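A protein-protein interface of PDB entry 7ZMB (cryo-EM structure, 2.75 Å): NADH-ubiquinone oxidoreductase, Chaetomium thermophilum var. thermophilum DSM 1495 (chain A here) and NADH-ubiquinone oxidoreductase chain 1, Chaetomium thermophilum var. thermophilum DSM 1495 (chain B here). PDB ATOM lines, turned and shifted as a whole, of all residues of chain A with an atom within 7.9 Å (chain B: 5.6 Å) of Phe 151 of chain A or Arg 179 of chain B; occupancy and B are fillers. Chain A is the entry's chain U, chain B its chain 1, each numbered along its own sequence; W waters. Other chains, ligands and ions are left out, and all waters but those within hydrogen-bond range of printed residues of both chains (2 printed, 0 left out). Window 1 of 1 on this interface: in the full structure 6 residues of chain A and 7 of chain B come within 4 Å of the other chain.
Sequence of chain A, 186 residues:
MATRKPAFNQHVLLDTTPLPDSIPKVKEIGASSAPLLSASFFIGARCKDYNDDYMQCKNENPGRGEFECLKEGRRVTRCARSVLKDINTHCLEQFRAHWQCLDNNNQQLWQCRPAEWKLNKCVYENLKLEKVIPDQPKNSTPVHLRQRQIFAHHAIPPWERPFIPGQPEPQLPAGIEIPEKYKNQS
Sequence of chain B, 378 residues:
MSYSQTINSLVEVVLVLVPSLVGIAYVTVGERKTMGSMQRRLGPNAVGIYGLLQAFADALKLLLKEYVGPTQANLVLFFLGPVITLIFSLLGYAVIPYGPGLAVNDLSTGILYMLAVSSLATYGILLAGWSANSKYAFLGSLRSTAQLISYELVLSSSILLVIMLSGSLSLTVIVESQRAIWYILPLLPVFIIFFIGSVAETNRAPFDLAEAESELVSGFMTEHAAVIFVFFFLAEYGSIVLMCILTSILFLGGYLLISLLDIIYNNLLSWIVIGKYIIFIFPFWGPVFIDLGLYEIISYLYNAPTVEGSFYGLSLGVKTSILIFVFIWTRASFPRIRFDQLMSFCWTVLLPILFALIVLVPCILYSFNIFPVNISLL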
ATOM      1  N   GLN A 108     -13.102  17.282  -8.054  1.00  0.00           N
ATOM      2  CA  GLN A 108     -13.302  16.724  -6.694  1.00  0.00           C
ATOM      3  C   GLN A 108     -13.347  15.201  -6.806  1.00  0.00           C
ATOM      4  O   GLN A 108     -14.199  14.697  -7.542  1.00  0.00           O
ATOM      5  CB  GLN A 108     -14.511  17.385  -6.034  1.00  0.00           C
ATOM      6  CG  GLN A 108     -14.344  18.893  -5.895  1.00  0.00           C
ATOM      7  CD  GLN A 108     -15.570  19.610  -5.388  1.00  0.00           C
ATOM      8  OE1 GLN A 108     -15.527  20.795  -5.069  1.00  0.00           O
ATOM      9  NE2 GLN A 108     -16.677  18.894  -5.305  1.00  0.00           N
ATOM     10  N   TRP A 110     -14.140  12.834  -4.617  1.00  0.00           N
ATOM     11  CA  TRP A 110     -15.331  12.209  -3.987  1.00  0.00           C
ATOM     12  C   TRP A 110     -16.531  12.261  -4.936  1.00  0.00           C
ATOM     13  O   TRP A 110     -17.492  11.530  -4.691  1.00  0.00           O
ATOM     14  CB  TRP A 110     -15.632  12.838  -2.624  1.00  0.00           C
ATOM     15  CG  TRP A 110     -15.970  14.296  -2.636  1.00  0.00           C
ATOM     16  CD1 TRP A 110     -17.212  14.855  -2.714  1.00  0.00           C
ATOM     17  CD2 TRP A 110     -15.045  15.389  -2.511  1.00  0.00           C
ATOM     18  NE1 TRP A 110     -17.122  16.219  -2.665  1.00  0.00           N
ATOM     19  CE2 TRP A 110     -15.806  16.575  -2.536  1.00  0.00           C
ATOM     20  CE3 TRP A 110     -13.656  15.480  -2.383  1.00  0.00           C
ATOM     21  CZ2 TRP A 110     -15.218  17.833  -2.445  1.00  0.00           C
ATOM     22  CZ3 TRP A 110     -13.079  16.724  -2.291  1.00  0.00           C
ATOM     23  CH2 TRP A 110     -13.850  17.883  -2.325  1.00  0.00           C
ATOM     24  N   GLN A 111     -16.496  13.132  -5.939  1.00  0.00           N
ATOM     25  CA  GLN A 111     -17.656  13.321  -6.843  1.00  0.00           C
ATOM     26  C   GLN A 111     -17.640  12.300  -7.988  1.00  0.00           C
ATOM     27  O   GLN A 111     -18.634  12.228  -8.713  1.00  0.00           O
ATOM     28  CB  GLN A 111     -17.635  14.763  -7.351  1.00  0.00           C
ATOM     29  CG  GLN A 111     -17.789  15.811  -6.266  1.00  0.00           C
ATOM     30  CD  GLN A 111     -19.217  15.908  -5.798  1.00  0.00           C
ATOM     31  OE1 GLN A 111     -20.060  15.095  -6.163  1.00  0.00           O
ATOM     32  NE2 GLN A 111     -19.498  16.911  -4.984  1.00  0.00           N
ATOM     33  N   VAL A 143     -11.589   6.872   3.269  1.00  0.00           N
ATOM     34  CA  VAL A 143     -12.635   7.708   2.601  1.00  0.00           C
ATOM     35  C   VAL A 143     -12.783   7.373   1.106  1.00  0.00           C
ATOM     36  O   VAL A 143     -13.869   7.588   0.566  1.00  0.00           O
ATOM     37  CB  VAL A 143     -12.436   9.213   2.878  1.00  0.00           C
ATOM     38  CG1 VAL A 143     -11.405   9.835   1.950  1.00  0.00           C
ATOM     39  CG2 VAL A 143     -13.747   9.980   2.834  1.00  0.00           C
ATOM     40  N   ARG A 148     -20.574   5.236   0.916  1.00  0.00           N
ATOM     41  CA  ARG A 148     -21.413   6.447   0.874  1.00  0.00           C
ATOM     42  C   ARG A 148     -20.510   7.677   0.962  1.00  0.00           C
ATOM     43  O   ARG A 148     -19.713   7.751   1.911  1.00  0.00           O
ATOM     44  CB  ARG A 148     -22.446   6.373   1.994  1.00  0.00           C
ATOM     45  CG  ARG A 148     -23.583   5.398   1.728  1.00  0.00           C
ATOM     46  CD  ARG A 148     -24.833   5.843   2.460  1.00  0.00           C
ATOM     47  NE  ARG A 148     -25.115   7.244   2.180  1.00  0.00           N
ATOM     48  CZ  ARG A 148     -26.144   7.919   2.676  1.00  0.00           C
ATOM     49  NH1 ARG A 148     -26.314   9.191   2.361  1.00  0.00           N
ATOM     50  NH2 ARG A 148     -27.000   7.319   3.484  1.00  0.00           N
ATOM     51  N   GLN A 149     -20.608   8.578  -0.015  1.00  0.00           N
ATOM     52  CA  GLN A 149     -19.834   9.836   0.079  1.00  0.00           C
ATOM     53  C   GLN A 149     -20.783  10.945   0.531  1.00  0.00           C
ATOM     54  O   GLN A 149     -21.714  11.238  -0.217  1.00  0.00           O
ATOM     55  CB  GLN A 149     -19.043  10.134  -1.193  1.00  0.00           C
ATOM     56  CG  GLN A 149     -17.968   9.105  -1.504  1.00  0.00           C
ATOM     57  CD  GLN A 149     -16.902   8.965  -0.445  1.00  0.00           C
ATOM     58  OE1 GLN A 149     -16.451   9.935   0.159  1.00  0.00           O
ATOM     59  NE2 GLN A 149     -16.460   7.738  -0.238  1.00  0.00           N
ATOM     60  N   ILE A 150     -20.510  11.581   1.671  1.00  0.00           N
ATOM     61  CA  ILE A 150     -21.464  12.589   2.224  1.00  0.00           C
ATOM     62  C   ILE A 150     -21.393  13.901   1.434  1.00  0.00           C
ATOM     63  O   ILE A 150     -22.423  14.605   1.394  1.00  0.00           O
ATOM     64  CB  ILE A 150     -21.070  12.869   3.691  1.00  0.00           C
ATOM     65  CG1 ILE A 150     -21.133  11.619   4.571  1.00  0.00           C
ATOM     66  CG2 ILE A 150     -21.876  14.011   4.291  1.00  0.00           C
ATOM     67  CD1 ILE A 150     -20.656  11.854   5.984  1.00  0.00           C
ATOM     68  N   PHE A 151     -20.288  14.175   0.740  1.00  0.00           N
ATOM     69  CA  PHE A 151     -20.163  15.490   0.061  1.00  0.00           C
ATOM     70  C   PHE A 151     -20.437  15.351  -1.439  1.00  0.00           C
ATOM     71  O   PHE A 151     -20.363  16.365  -2.149  1.00  0.00           O
ATOM     72  CB  PHE A 151     -18.874  16.197   0.491  1.00  0.00           C
ATOM     73  CG  PHE A 151     -18.857  16.579   1.947  1.00  0.00           C
ATOM     74  CD1 PHE A 151     -19.530  17.707   2.390  1.00  0.00           C
ATOM     75  CD2 PHE A 151     -18.191  15.802   2.878  1.00  0.00           C
ATOM     76  CE1 PHE A 151     -19.527  18.054   3.732  1.00  0.00           C
ATOM     77  CE2 PHE A 151     -18.191  16.149   4.219  1.00  0.00           C
ATOM     78  CZ  PHE A 151     -18.856  17.273   4.643  1.00  0.00           C
ATOM     79  N   ALA A 152     -20.790  14.144  -1.886  1.00  0.00           N
ATOM     80  CA  ALA A 152     -21.096  13.897  -3.316  1.00  0.00           C
ATOM     81  C   ALA A 152     -22.505  14.400  -3.631  1.00  0.00           C
ATOM     82  O   ALA A 152     -23.425  14.056  -2.877  1.00  0.00           O
ATOM     83  CB  ALA A 152     -20.981  12.434  -3.625  1.00  0.00           C
ATOM     84  N   HIS A 153     -22.655  15.181  -4.704  1.00  0.00           N
ATOM     85  CA  HIS A 153     -24.004  15.673  -5.095  1.00  0.00           C
ATOM     86  C   HIS A 153     -24.891  14.522  -5.563  1.00  0.00           C
ATOM     87  O   HIS A 153     -26.068  14.515  -5.201  1.00  0.00           O
ATOM     88  CB  HIS A 153     -23.932  16.865  -6.049  1.00  0.00           C
ATOM     89  CG  HIS A 153     -22.991  16.730  -7.187  1.00  0.00           C
ATOM     90  ND1 HIS A 153     -23.217  15.865  -8.231  1.00  0.00           N
ATOM     91  CD2 HIS A 153     -21.855  17.394  -7.476  1.00  0.00           C
ATOM     92  CE1 HIS A 153     -22.242  15.975  -9.105  1.00  0.00           C
ATOM     93  NE2 HIS A 153     -21.393  16.906  -8.662  1.00  0.00           N
ATOM     94  N   HIS A 154     -24.347  13.621  -6.381  1.00  0.00           N
ATOM     95  CA  HIS A 154     -25.111  12.420  -6.796  1.00  0.00           C
ATOM     96  C   HIS A 154     -24.668  11.251  -5.930  1.00  0.00           C
ATOM     97  O   HIS A 154     -23.457  10.967  -5.895  1.00  0.00           O
ATOM     98  CB  HIS A 154     -24.951  12.138  -8.288  1.00  0.00           C
ATOM     99  CG  HIS A 154     -25.788  13.020  -9.150  1.00  0.00           C
ATOM    100  ND1 HIS A 154     -25.380  14.284  -9.532  1.00  0.00           N
ATOM    101  CD2 HIS A 154     -27.006  12.832  -9.703  1.00  0.00           C
ATOM    102  CE1 HIS A 154     -26.310  14.836 -10.285  1.00  0.00           C
ATOM    103  NE2 HIS A 154     -27.318  13.963 -10.405  1.00  0.00           N
ATOM    104  N   ILE A 156     -23.622   7.762  -4.423  1.00  0.00           N
ATOM    105  CA  ILE A 156     -22.912   6.607  -5.036  1.00  0.00           C
ATOM    106  C   ILE A 156     -23.955   5.506  -5.181  1.00  0.00           C
ATOM    107  O   ILE A 156     -24.695   5.262  -4.222  1.00  0.00           O
ATOM    108  CB  ILE A 156     -21.683   6.176  -4.197  1.00  0.00           C
ATOM    109  CG1 ILE A 156     -20.482   7.091  -4.436  1.00  0.00           C
ATOM    110  CG2 ILE A 156     -21.318   4.726  -4.469  1.00  0.00           C
ATOM    111  CD1 ILE A 156     -20.640   8.468  -3.861  1.00  0.00           C
ATOM    112  N   PRO B 100     -23.428  25.805  -6.745  1.00  0.00           N
ATOM    113  CA  PRO B 100     -22.045  25.808  -6.248  1.00  0.00           C
ATOM    114  C   PRO B 100     -21.166  26.767  -7.027  1.00  0.00           C
ATOM    115  O   PRO B 100     -20.775  26.489  -8.163  1.00  0.00           O
ATOM    116  CB  PRO B 100     -21.603  24.353  -6.437  1.00  0.00           C
ATOM    117  CG  PRO B 100     -22.860  23.582  -6.604  1.00  0.00           C
ATOM    118  CD  PRO B 100     -23.821  24.491  -7.263  1.00  0.00           C
ATOM    119  N   VAL B 175     -22.254  26.483   2.307  1.00  0.00           N
ATOM    120  CA  VAL B 175     -23.395  25.674   1.801  1.00  0.00           C
ATOM    121  C   VAL B 175     -22.930  24.233   1.575  1.00  0.00           C
ATOM    122  O   VAL B 175     -23.655  23.311   1.991  1.00  0.00           O
ATOM    123  CB  VAL B 175     -24.000  26.294   0.528  1.00  0.00           C
ATOM    124  CG1 VAL B 175     -25.118  25.423  -0.014  1.00  0.00           C
ATOM    125  CG2 VAL B 175     -24.499  27.709   0.762  1.00  0.00           C
ATOM    126  N   GLU B 176     -21.762  24.063   0.957  1.00  0.00           N
ATOM    127  CA  GLU B 176     -21.183  22.722   0.682  1.00  0.00           C
ATOM    128  C   GLU B 176     -20.953  21.971   1.997  1.00  0.00           C
ATOM    129  O   GLU B 176     -21.191  20.762   2.035  1.00  0.00           O
ATOM    130  CB  GLU B 176     -19.935  22.890  -0.187  1.00  0.00           C
ATOM    131  CG  GLU B 176     -20.257  23.322  -1.604  1.00  0.00           C
ATOM    132  CD  GLU B 176     -21.122  22.331  -2.361  1.00  0.00           C
ATOM    133  OE1 GLU B 176     -21.949  22.771  -3.176  1.00  0.00           O
ATOM    134  OE2 GLU B 176     -20.956  21.120  -2.142  1.00  0.00           O
ATOM    135  N   SER B 177     -20.500  22.677   3.028  1.00  0.00           N
ATOM    136  CA  SER B 177     -20.239  22.068   4.359  1.00  0.00           C
ATOM    137  C   SER B 177     -21.539  21.503   4.946  1.00  0.00           C
ATOM    138  O   SER B 177     -21.465  20.490   5.642  1.00  0.00           O
ATOM    139  CB  SER B 177     -19.562  23.061   5.274  1.00  0.00           C
ATOM    140  OG  SER B 177     -18.338  23.512   4.722  1.00  0.00           O
ATOM    141  N   GLN B 178     -22.676  22.142   4.680  1.00  0.00           N
ATOM    142  CA  GLN B 178     -24.004  21.717   5.195  1.00  0.00           C
ATOM    143  C   GLN B 178     -24.523  20.458   4.482  1.00  0.00           C
ATOM    144  O   GLN B 178     -25.637  20.045   4.804  1.00  0.00           O
ATOM    145  CB  GLN B 178     -24.944  22.919   5.199  1.00  0.00           C
ATOM    146  CG  GLN B 178     -24.471  24.051   6.092  1.00  0.00           C
ATOM    147  CD  GLN B 178     -25.363  25.264   6.012  1.00  0.00           C
ATOM    148  OE1 GLN B 178     -26.410  25.331   6.648  1.00  0.00           O
ATOM    149  NE2 GLN B 178     -24.942  26.243   5.232  1.00  0.00           N
ATOM    150  N   ARG B 179     -23.766  19.873   3.548  1.00  0.00           N
ATOM    151  CA  ARG B 179     -24.167  18.565   2.953  1.00  0.00           C
ATOM    152  C   ARG B 179     -24.013  17.515   4.059  1.00  0.00           C
ATOM    153  O   ARG B 179     -24.565  16.416   3.911  1.00  0.00           O
ATOM    154  CB  ARG B 179     -23.394  18.222   1.674  1.00  0.00           C
ATOM    155  CG  ARG B 179     -23.666  19.137   0.493  1.00  0.00           C
ATOM    156  CD  ARG B 179     -22.891  18.671  -0.719  1.00  0.00           C
ATOM    157  NE  ARG B 179     -23.169  19.483  -1.891  1.00  0.00           N
ATOM    158  CZ  ARG B 179     -24.079  19.206  -2.811  1.00  0.00           C
ATOM    159  NH1 ARG B 179     -24.817  18.116  -2.707  1.00  0.00           N
ATOM    160  NH2 ARG B 179     -24.253  20.028  -3.830  1.00  0.00           N
ATOM    161  N   ALA B 180     -23.309  17.858   5.138  1.00  0.00           N
ATOM    162  CA  ALA B 180     -23.173  16.962   6.305  1.00  0.00           C
ATOM    163  C   ALA B 180     -24.422  17.099   7.178  1.00  0.00           C
ATOM    164  O   ALA B 180     -24.988  16.064   7.548  1.00  0.00           O
ATOM    165  CB  ALA B 180     -21.957  17.404   7.066  1.00  0.00           C
ATOM    166  N   ILE B 181     -24.827  18.323   7.498  1.00  0.00           N
ATOM    167  CA  ILE B 181     -26.063  18.584   8.222  1.00  0.00           C
ATOM    168  C   ILE B 181     -26.338  20.065   8.033  1.00  0.00           C
ATOM    169  O   ILE B 181     -25.405  20.864   7.918  1.00  0.00           O
ATOM    170  CB  ILE B 181     -25.962  18.201   9.717  1.00  0.00           C
ATOM    171  CG1 ILE B 181     -27.330  18.240  10.404  1.00  0.00           C
ATOM    172  CG2 ILE B 181     -25.021  19.120  10.455  1.00  0.00           C
ATOM    173  CD1 ILE B 181     -28.348  17.328   9.805  1.00  0.00           C
ATOM    174  N   TYR B 255     -28.740  26.373  -1.289  1.00  0.00           N
ATOM    175  CA  TYR B 255     -29.402  25.790  -2.448  1.00  0.00           C
ATOM    176  C   TYR B 255     -29.583  24.281  -2.343  1.00  0.00           C
ATOM    177  O   TYR B 255     -30.143  23.681  -3.261  1.00  0.00           O
ATOM    178  CB  TYR B 255     -28.611  26.116  -3.721  1.00  0.00           C
ATOM    179  CG  TYR B 255     -27.130  25.865  -3.585  1.00  0.00           C
ATOM    180  CD1 TYR B 255     -26.606  24.596  -3.765  1.00  0.00           C
ATOM    181  CD2 TYR B 255     -26.257  26.893  -3.276  1.00  0.00           C
ATOM    182  CE1 TYR B 255     -25.271  24.359  -3.636  1.00  0.00           C
ATOM    183  CE2 TYR B 255     -24.910  26.661  -3.152  1.00  0.00           C
ATOM    184  CZ  TYR B 255     -24.427  25.391  -3.325  1.00  0.00           C
ATOM    185  OH  TYR B 255     -23.090  25.152  -3.196  1.00  0.00           O
ATOM    186  N   LEU B 256     -29.121  23.659  -1.262  1.00  0.00           N
ATOM    187  CA  LEU B 256     -29.157  22.207  -1.149  1.00  0.00           C
ATOM    188  C   LEU B 256     -30.579  21.676  -1.259  1.00  0.00           C
ATOM    189  O   LEU B 256     -31.512  22.215  -0.658  1.00  0.00           O
ATOM    190  CB  LEU B 256     -28.547  21.768   0.179  1.00  0.00           C
ATOM    191  CG  LEU B 256     -27.026  21.769   0.276  1.00  0.00           C
ATOM    192  CD1 LEU B 256     -26.605  21.032   1.511  1.00  0.00           C
ATOM    193  CD2 LEU B 256     -26.404  21.180  -0.968  1.00  0.00           C
ATOM    194  N   TYR B 312     -31.394  23.731  -7.835  1.00  0.00           N
ATOM    195  CA  TYR B 312     -30.713  24.575  -6.859  1.00  0.00           C
ATOM    196  C   TYR B 312     -31.436  25.906  -6.686  1.00  0.00           C
ATOM    197  O   TYR B 312     -31.643  26.367  -5.561  1.00  0.00           O
ATOM    198  CB  TYR B 312     -29.266  24.809  -7.286  1.00  0.00           C
ATOM    199  CG  TYR B 312     -28.334  23.651  -7.025  1.00  0.00           C
ATOM    200  CD1 TYR B 312     -28.509  22.822  -5.931  1.00  0.00           C
ATOM    201  CD2 TYR B 312     -27.281  23.388  -7.878  1.00  0.00           C
ATOM    202  CE1 TYR B 312     -27.656  21.772  -5.694  1.00  0.00           C
ATOM    203  CE2 TYR B 312     -26.428  22.339  -7.653  1.00  0.00           C
ATOM    204  CZ  TYR B 312     -26.612  21.538  -6.564  1.00  0.00           C
ATOM    205  OH  TYR B 312     -25.746  20.494  -6.354  1.00  0.00           O
ATOM    206  N   LEU B 378     -14.148  22.285  -0.495  1.00  0.00           N
ATOM    207  CA  LEU B 378     -15.545  22.276  -0.991  1.00  0.00           C
ATOM    208  C   LEU B 378     -15.849  23.639  -1.633  1.00  0.00           C
ATOM    209  O   LEU B 378     -16.156  23.650  -2.829  1.00  0.00           O
ATOM    210  CB  LEU B 378     -16.460  22.016   0.212  1.00  0.00           C
ATOM    211  CG  LEU B 378     -16.135  20.786   1.055  1.00  0.00           C
ATOM    212  CD1 LEU B 378     -16.928  20.799   2.351  1.00  0.00           C
ATOM    213  CD2 LEU B 378     -16.419  19.511   0.283  1.00  0.00           C
HETATM  214  O   HOH W   1     -24.275  15.847  -1.064  1.00  0.00           O
HETATM  215  O   HOH W   2     -19.141  19.009  -2.491  1.00  0.00           O
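Printed residues of chain B within 4 Å of Ile 150 of chain A: Arg 179 and Ala 180. Of chain B, only Glu 176, Ser 177, Arg 179 and Ala 180 come within 4 Å of Phe 151 of chain A. Ala 152 of chain A touches none of the printed residues of chain B. Of the printed residues of chain B, His 153 of chain A touches Arg 179 (3.5 Å). Printed residues of chain A within 4 Å of Ser 177 of chain B: Phe 151 (3.7 Å). Of chain A, only Ile 150 (3.6 Å), Phe 151 (3.7 Å) and His 153 (3.5 Å) come within 4 Å of Arg 179 of chain B. Printed residues of chain A within 4 Å of Leu 378 of chain B: Gln 108 and Trp 110. The nearest residue of chain B that does not touch Phe 151 of chain A is Leu 378 of chain B (4.02 Å). The nearest printed residue of chain B that does not touch Ile 150 of chain A is Ile 181 of chain B (6.1 Å).
Among the printed residues, merely in contact across the chains: Gln 108 of chain A with Leu 378 of chain B, Trp 110 of chain A with Leu 378 of chain B, Ile 150 of chain A with Arg 179 of chain B, Ile 150 of chain A with Ala 180 of chain B, Phe 151 of chain A with Glu 176 of chain B, Phe 151 of chain A with Ser 177 of chain B, Phe 151 of chain A with Arg 179 of chain B, Phe 151 of chain A with Ala 180 of chain B and His 153 of chain A with Arg 179 of chain B.
Water W1 lies within hydrogen-bond range of O of Ala 152 of chain A (2.7 Å), NH1 of Arg 179 of chain B (2.9 Å) and O of Ile 150 of chain A (3.3 Å). Water W2 lies within hydrogen-bond range of OE2 of Glu 176 of chain B (2.8 Å), O of Phe 151 of chain A (2.9 Å), NE2 of Gln 111 of chain A (3.3 Å) and NE1 of Trp 110 of chain A (3.4 Å).
O of Phe 151 of chain A sits at hydrogen-bond distance from NE1 of Trp 110 of chain A (3.3 Å). NE2 of Gln 108 of chain A lies close to NE2 of Gln 111 of chain A (3.5 Å). The side-chain carboxylate (OE2) of Glu 176 of chain B is in salt-bridge range of the guanidinium group (NE) of Arg 179 of chain B. ND1 of His 153 of chain A lies within hydrogen-bond range of ND1 of His 154 of chain A (3.0 Å). The backbone NH (N) of His 153 of chain A lies within hydrogen-bond range of the side-chain amide oxygen (OE1) of Gln 111 of chain A (3.0 Å). OH of Tyr 255 of chain B sits at hydrogen-bond distance from OE1 of Glu 176 of chain B, at 2.6 Å.
Of the 12 printed residues of chain A, 5 touch a printed residue of chain B. Printed residues of chain A that touch a printed residue of chain B: Gln 108, Trp 110, Ile 150, Phe 151 and His 153. Printed residues of chain B that touch a printed residue of chain A: Glu 176, Ser 177, Arg 179, Ala 180 and Leu 378. Hydrophobic or aromatic side chains of chain B that line the printed part of chain A: Ala 180 and Leu 378. Among the printed residues, 9 pairs touch across the chains. Among the printed residues, no Asp or Glu carboxylate lies within 4 Å of a Lys or Arg side-chain nitrogen of the other chain.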
